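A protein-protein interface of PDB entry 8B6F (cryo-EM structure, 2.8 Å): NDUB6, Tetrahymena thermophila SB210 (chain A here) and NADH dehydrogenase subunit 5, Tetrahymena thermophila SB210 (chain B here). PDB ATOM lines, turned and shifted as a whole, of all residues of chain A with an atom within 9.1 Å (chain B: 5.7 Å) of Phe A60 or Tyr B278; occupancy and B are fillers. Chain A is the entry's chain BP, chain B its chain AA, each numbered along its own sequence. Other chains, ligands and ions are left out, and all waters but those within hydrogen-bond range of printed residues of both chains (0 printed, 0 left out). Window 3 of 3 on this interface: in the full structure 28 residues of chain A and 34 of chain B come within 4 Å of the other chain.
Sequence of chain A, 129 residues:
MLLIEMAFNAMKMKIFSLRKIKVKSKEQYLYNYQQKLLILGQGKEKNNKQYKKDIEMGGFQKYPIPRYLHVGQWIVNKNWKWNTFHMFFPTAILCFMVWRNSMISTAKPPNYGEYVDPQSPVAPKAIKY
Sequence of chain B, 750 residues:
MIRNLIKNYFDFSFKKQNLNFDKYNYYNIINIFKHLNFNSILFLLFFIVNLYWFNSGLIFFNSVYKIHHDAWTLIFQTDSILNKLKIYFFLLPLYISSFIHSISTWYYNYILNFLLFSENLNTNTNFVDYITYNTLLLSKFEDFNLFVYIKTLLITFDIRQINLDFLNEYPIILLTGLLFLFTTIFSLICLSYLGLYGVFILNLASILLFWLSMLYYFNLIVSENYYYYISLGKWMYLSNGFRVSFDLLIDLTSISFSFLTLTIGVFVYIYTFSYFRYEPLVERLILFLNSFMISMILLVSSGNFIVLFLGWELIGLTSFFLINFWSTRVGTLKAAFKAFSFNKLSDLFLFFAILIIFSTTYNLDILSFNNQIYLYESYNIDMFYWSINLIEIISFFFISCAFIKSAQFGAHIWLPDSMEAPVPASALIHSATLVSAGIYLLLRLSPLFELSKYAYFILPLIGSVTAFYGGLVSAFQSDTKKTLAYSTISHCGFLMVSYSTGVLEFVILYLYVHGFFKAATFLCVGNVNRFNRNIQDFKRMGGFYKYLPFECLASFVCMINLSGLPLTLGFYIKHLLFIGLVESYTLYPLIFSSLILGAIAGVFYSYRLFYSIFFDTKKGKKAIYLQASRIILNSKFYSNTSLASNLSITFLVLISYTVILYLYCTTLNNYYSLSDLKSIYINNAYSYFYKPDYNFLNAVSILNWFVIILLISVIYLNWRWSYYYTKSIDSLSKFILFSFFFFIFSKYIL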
ATOM      1  N   GLY A  58     -13.313   5.292 -13.832  1.00  0.00           N
ATOM      2  CA  GLY A  58     -13.170   6.024 -12.543  1.00  0.00           C
ATOM      3  C   GLY A  58     -11.771   6.567 -12.334  1.00  0.00           C
ATOM      4  O   GLY A  58     -11.553   7.778 -12.362  1.00  0.00           O
ATOM      5  N   GLY A  59     -10.817   5.666 -12.114  1.00  0.00           N
ATOM      6  CA  GLY A  59      -9.435   6.052 -11.949  1.00  0.00           C
ATOM      7  C   GLY A  59      -8.749   6.300 -13.278  1.00  0.00           C
ATOM      8  O   GLY A  59      -9.305   6.096 -14.357  1.00  0.00           O
ATOM      9  N   PHE A  60      -7.505   6.755 -13.187  1.00  0.00           N
ATOM     10  CA  PHE A  60      -6.721   7.032 -14.380  1.00  0.00           C
ATOM     11  C   PHE A  60      -6.297   5.731 -15.054  1.00  0.00           C
ATOM     12  O   PHE A  60      -6.196   4.679 -14.418  1.00  0.00           O
ATOM     13  CB  PHE A  60      -5.493   7.867 -14.021  1.00  0.00           C
ATOM     14  CG  PHE A  60      -4.768   8.419 -15.211  1.00  0.00           C
ATOM     15  CD1 PHE A  60      -5.286   9.490 -15.915  1.00  0.00           C
ATOM     16  CD2 PHE A  60      -3.558   7.880 -15.611  1.00  0.00           C
ATOM     17  CE1 PHE A  60      -4.620  10.007 -17.006  1.00  0.00           C
ATOM     18  CE2 PHE A  60      -2.885   8.392 -16.701  1.00  0.00           C
ATOM     19  CZ  PHE A  60      -3.416   9.458 -17.399  1.00  0.00           C
ATOM     20  N   GLN A  61      -6.057   5.811 -16.359  1.00  0.00           N
ATOM     21  CA  GLN A  61      -5.620   4.643 -17.110  1.00  0.00           C
ATOM     22  C   GLN A  61      -4.231   4.211 -16.659  1.00  0.00           C
ATOM     23  O   GLN A  61      -3.349   5.041 -16.426  1.00  0.00           O
ATOM     24  CB  GLN A  61      -5.614   4.944 -18.608  1.00  0.00           C
ATOM     25  CG  GLN A  61      -5.157   3.777 -19.471  1.00  0.00           C
ATOM     26  CD  GLN A  61      -5.210   4.095 -20.947  1.00  0.00           C
ATOM     27  OE1 GLN A  61      -5.851   5.058 -21.362  1.00  0.00           O
ATOM     28  NE2 GLN A  61      -4.528   3.290 -21.751  1.00  0.00           N
ATOM     29  N   LYS A  62      -4.038   2.901 -16.542  1.00  0.00           N
ATOM     30  CA  LYS A  62      -2.760   2.377 -16.089  1.00  0.00           C
ATOM     31  C   LYS A  62      -1.707   2.508 -17.183  1.00  0.00           C
ATOM     32  O   LYS A  62      -1.982   2.283 -18.364  1.00  0.00           O
ATOM     33  CB  LYS A  62      -2.911   0.918 -15.665  1.00  0.00           C
ATOM     34  CG  LYS A  62      -3.962   0.724 -14.586  1.00  0.00           C
ATOM     35  CD  LYS A  62      -3.999  -0.694 -14.049  1.00  0.00           C
ATOM     36  CE  LYS A  62      -5.051  -0.811 -12.958  1.00  0.00           C
ATOM     37  NZ  LYS A  62      -5.146  -2.180 -12.394  1.00  0.00           N
ATOM     38  N   TYR A  63      -0.498   2.879 -16.781  1.00  0.00           N
ATOM     39  CA  TYR A  63       0.624   3.060 -17.683  1.00  0.00           C
ATOM     40  C   TYR A  63       1.843   2.329 -17.142  1.00  0.00           C
ATOM     41  O   TYR A  63       1.951   2.107 -15.932  1.00  0.00           O
ATOM     42  CB  TYR A  63       0.951   4.549 -17.865  1.00  0.00           C
ATOM     43  CG  TYR A  63       1.065   5.311 -16.568  1.00  0.00           C
ATOM     44  CD1 TYR A  63       2.269   5.374 -15.881  1.00  0.00           C
ATOM     45  CD2 TYR A  63      -0.030   5.973 -16.033  1.00  0.00           C
ATOM     46  CE1 TYR A  63       2.377   6.071 -14.695  1.00  0.00           C
ATOM     47  CE2 TYR A  63       0.069   6.672 -14.847  1.00  0.00           C
ATOM     48  CZ  TYR A  63       1.275   6.717 -14.183  1.00  0.00           C
ATOM     49  OH  TYR A  63       1.380   7.413 -13.002  1.00  0.00           O
ATOM     50  N   PRO A  64       2.772   1.937 -18.013  1.00  0.00           N
ATOM     51  CA  PRO A  64       3.935   1.170 -17.549  1.00  0.00           C
ATOM     52  C   PRO A  64       4.800   1.961 -16.579  1.00  0.00           C
ATOM     53  O   PRO A  64       4.958   3.177 -16.696  1.00  0.00           O
ATOM     54  CB  PRO A  64       4.693   0.854 -18.845  1.00  0.00           C
ATOM     55  CG  PRO A  64       4.233   1.876 -19.817  1.00  0.00           C
ATOM     56  CD  PRO A  64       2.810   2.162 -19.467  1.00  0.00           C
ATOM     57  N   TRP A  74       0.621   1.196  -8.325  1.00  0.00           N
ATOM     58  CA  TRP A  74      -0.096  -0.051  -8.590  1.00  0.00           C
ATOM     59  C   TRP A  74       0.707  -1.268  -8.135  1.00  0.00           C
ATOM     60  O   TRP A  74       0.858  -2.251  -8.864  1.00  0.00           O
ATOM     61  CB  TRP A  74      -0.454  -0.167 -10.071  1.00  0.00           C
ATOM     62  CG  TRP A  74      -1.528   0.772 -10.513  1.00  0.00           C
ATOM     63  CD1 TRP A  74      -2.841   0.739 -10.151  1.00  0.00           C
ATOM     64  CD2 TRP A  74      -1.386   1.878 -11.412  1.00  0.00           C
ATOM     65  NE1 TRP A  74      -3.526   1.757 -10.764  1.00  0.00           N
ATOM     66  CE2 TRP A  74      -2.656   2.473 -11.542  1.00  0.00           C
ATOM     67  CE3 TRP A  74      -0.309   2.424 -12.114  1.00  0.00           C
ATOM     68  CZ2 TRP A  74      -2.878   3.585 -12.350  1.00  0.00           C
ATOM     69  CZ3 TRP A  74      -0.530   3.530 -12.914  1.00  0.00           C
ATOM     70  CH2 TRP A  74      -1.805   4.100 -13.025  1.00  0.00           C
ATOM     71  N   PHE B 276     -10.653   6.401  -3.972  1.00  0.00           N
ATOM     72  CA  PHE B 276      -9.406   6.325  -4.715  1.00  0.00           C
ATOM     73  C   PHE B 276      -9.268   5.007  -5.461  1.00  0.00           C
ATOM     74  O   PHE B 276      -8.152   4.591  -5.785  1.00  0.00           O
ATOM     75  CB  PHE B 276      -8.222   6.544  -3.771  1.00  0.00           C
ATOM     76  CG  PHE B 276      -7.409   7.757  -4.104  1.00  0.00           C
ATOM     77  CD1 PHE B 276      -7.996   9.012  -4.134  1.00  0.00           C
ATOM     78  CD2 PHE B 276      -6.059   7.646  -4.384  1.00  0.00           C
ATOM     79  CE1 PHE B 276      -7.253  10.130  -4.442  1.00  0.00           C
ATOM     80  CE2 PHE B 276      -5.310   8.762  -4.693  1.00  0.00           C
ATOM     81  CZ  PHE B 276      -5.908  10.006  -4.721  1.00  0.00           C
ATOM     82  N   ARG B 277     -10.390   4.352  -5.737  1.00  0.00           N
ATOM     83  CA  ARG B 277     -10.397   3.095  -6.466  1.00  0.00           C
ATOM     84  C   ARG B 277      -9.717   3.254  -7.820  1.00  0.00           C
ATOM     85  O   ARG B 277      -9.986   4.206  -8.557  1.00  0.00           O
ATOM     86  CB  ARG B 277     -11.848   2.649  -6.635  1.00  0.00           C
ATOM     87  CG  ARG B 277     -12.067   1.317  -7.304  1.00  0.00           C
ATOM     88  CD  ARG B 277     -13.462   1.277  -7.904  1.00  0.00           C
ATOM     89  NE  ARG B 277     -14.442   1.908  -7.026  1.00  0.00           N
ATOM     90  CZ  ARG B 277     -15.615   2.380  -7.421  1.00  0.00           C
ATOM     91  NH1 ARG B 277     -16.000   2.309  -8.684  1.00  0.00           N
ATOM     92  NH2 ARG B 277     -16.422   2.945  -6.528  1.00  0.00           N
ATOM     93  N   TYR B 278      -8.830   2.311  -8.147  1.00  0.00           N
ATOM     94  CA  TYR B 278      -8.119   2.284  -9.425  1.00  0.00           C
ATOM     95  C   TYR B 278      -7.150   3.453  -9.575  1.00  0.00           C
ATOM     96  O   TYR B 278      -6.845   3.868 -10.693  1.00  0.00           O
ATOM     97  CB  TYR B 278      -9.093   2.274 -10.606  1.00  0.00           C
ATOM     98  CG  TYR B 278     -10.165   1.221 -10.506  1.00  0.00           C
ATOM     99  CD1 TYR B 278      -9.929   0.016  -9.858  1.00  0.00           C
ATOM    100  CD2 TYR B 278     -11.418   1.434 -11.061  1.00  0.00           C
ATOM    101  CE1 TYR B 278     -10.911  -0.946  -9.764  1.00  0.00           C
ATOM    102  CE2 TYR B 278     -12.406   0.480 -10.972  1.00  0.00           C
ATOM    103  CZ  TYR B 278     -12.148  -0.708 -10.321  1.00  0.00           C
ATOM    104  OH  TYR B 278     -13.130  -1.664 -10.235  1.00  0.00           O
ATOM    105  N   GLU B 279      -6.660   3.983  -8.473  1.00  0.00           N
ATOM    106  CA  GLU B 279      -5.701   5.070  -8.537  1.00  0.00           C
ATOM    107  C   GLU B 279      -4.282   4.541  -8.374  1.00  0.00           C
ATOM    108  O   GLU B 279      -4.068   3.505  -7.736  1.00  0.00           O
ATOM    109  CB  GLU B 279      -5.982   6.103  -7.444  1.00  0.00           C
ATOM    110  CG  GLU B 279      -7.299   6.841  -7.613  1.00  0.00           C
ATOM    111  CD  GLU B 279      -7.274   7.825  -8.761  1.00  0.00           C
ATOM    112  OE1 GLU B 279      -6.221   7.951  -9.418  1.00  0.00           O
ATOM    113  OE2 GLU B 279      -8.307   8.482  -9.003  1.00  0.00           O
ATOM    114  N   PRO B 280      -3.285   5.228  -8.937  1.00  0.00           N
ATOM    115  CA  PRO B 280      -1.905   4.737  -8.796  1.00  0.00           C
ATOM    116  C   PRO B 280      -1.461   4.612  -7.353  1.00  0.00           C
ATOM    117  O   PRO B 280      -0.726   3.678  -7.011  1.00  0.00           O
ATOM    118  CB  PRO B 280      -1.075   5.788  -9.548  1.00  0.00           C
ATOM    119  CG  PRO B 280      -2.035   6.537 -10.384  1.00  0.00           C
ATOM    120  CD  PRO B 280      -3.348   6.493  -9.685  1.00  0.00           C
ATOM    121  N   VAL B 282      -3.059   4.528  -3.758  1.00  0.00           N
ATOM    122  CA  VAL B 282      -4.093   4.424  -2.739  1.00  0.00           C
ATOM    123  C   VAL B 282      -3.487   4.181  -1.364  1.00  0.00           C
ATOM    124  O   VAL B 282      -3.989   4.690  -0.362  1.00  0.00           O
ATOM    125  CB  VAL B 282      -5.099   3.313  -3.108  1.00  0.00           C
ATOM    126  CG1 VAL B 282      -6.236   3.262  -2.097  1.00  0.00           C
ATOM    127  CG2 VAL B 282      -5.635   3.528  -4.510  1.00  0.00           C
ATOM    128  N   ARG B 530     -16.889  11.949  -8.081  1.00  0.00           N
ATOM    129  CA  ARG B 530     -16.286  10.818  -8.774  1.00  0.00           C
ATOM    130  C   ARG B 530     -17.156  10.355  -9.936  1.00  0.00           C
ATOM    131  O   ARG B 530     -16.643  10.042 -11.016  1.00  0.00           O
ATOM    132  CB  ARG B 530     -16.040   9.670  -7.796  1.00  0.00           C
ATOM    133  CG  ARG B 530     -15.404   8.456  -8.448  1.00  0.00           C
ATOM    134  CD  ARG B 530     -14.966   7.422  -7.430  1.00  0.00           C
ATOM    135  NE  ARG B 530     -14.393   6.252  -8.083  1.00  0.00           N
ATOM    136  CZ  ARG B 530     -13.132   6.152  -8.480  1.00  0.00           C
ATOM    137  NH1 ARG B 530     -12.269   7.139  -8.300  1.00  0.00           N
ATOM    138  NH2 ARG B 530     -12.725   5.034  -9.073  1.00  0.00           N
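Arg B530 touches Gly A58. Gly A59 touches Arg B277. O of Tyr B278 touches CA of Gly A59, at 3.6 Å. CA of Gly A59 touches OE2 of Glu B279, 3.98 Å away. Arg B530 touches Gly A59 (NH2 to N, 3.6 Å). Tyr B278 touches Phe A60. Trp A74 touches Tyr B278 (NE1 to O, 3.9 Å). O of Glu B279 touches NE1 of Trp A74, at 3.5 Å.
The backbone NH of Trp A74 lies within hydrogen-bond range of the backbone carbonyl oxygen of Pro B280 (3.1 Å).
Tyr B278 touches just these residues of chain A: Gly A59, Phe A60 and Trp A74. Printed residues of chain B within 4 Å of Trp A74: Tyr B278 (3.9 Å), Glu B279 (3.5 Å) and Pro B280 (3.1 Å). Of the printed residues of chain A, Arg B530 touches Gly A58 and Gly A59. Of the printed residues of chain B, Gly A58 touches Arg B530. The nearest residue of chain A that does not touch Tyr B278 is Gly A58 (5.1 Å).
The backbone carbonyl oxygen of Arg B277 sits at hydrogen-bond distance from the guanidinium group of Arg B530, at 2.9 Å.
Of the 7 printed residues of chain B, 5 touch a printed residue of chain A. Printed residues of chain B that touch a printed residue of chain A: Arg B277, Tyr B278, Glu B279, Pro B280 and Arg B530. Among the printed residues, 9 pairs touch across the chains.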
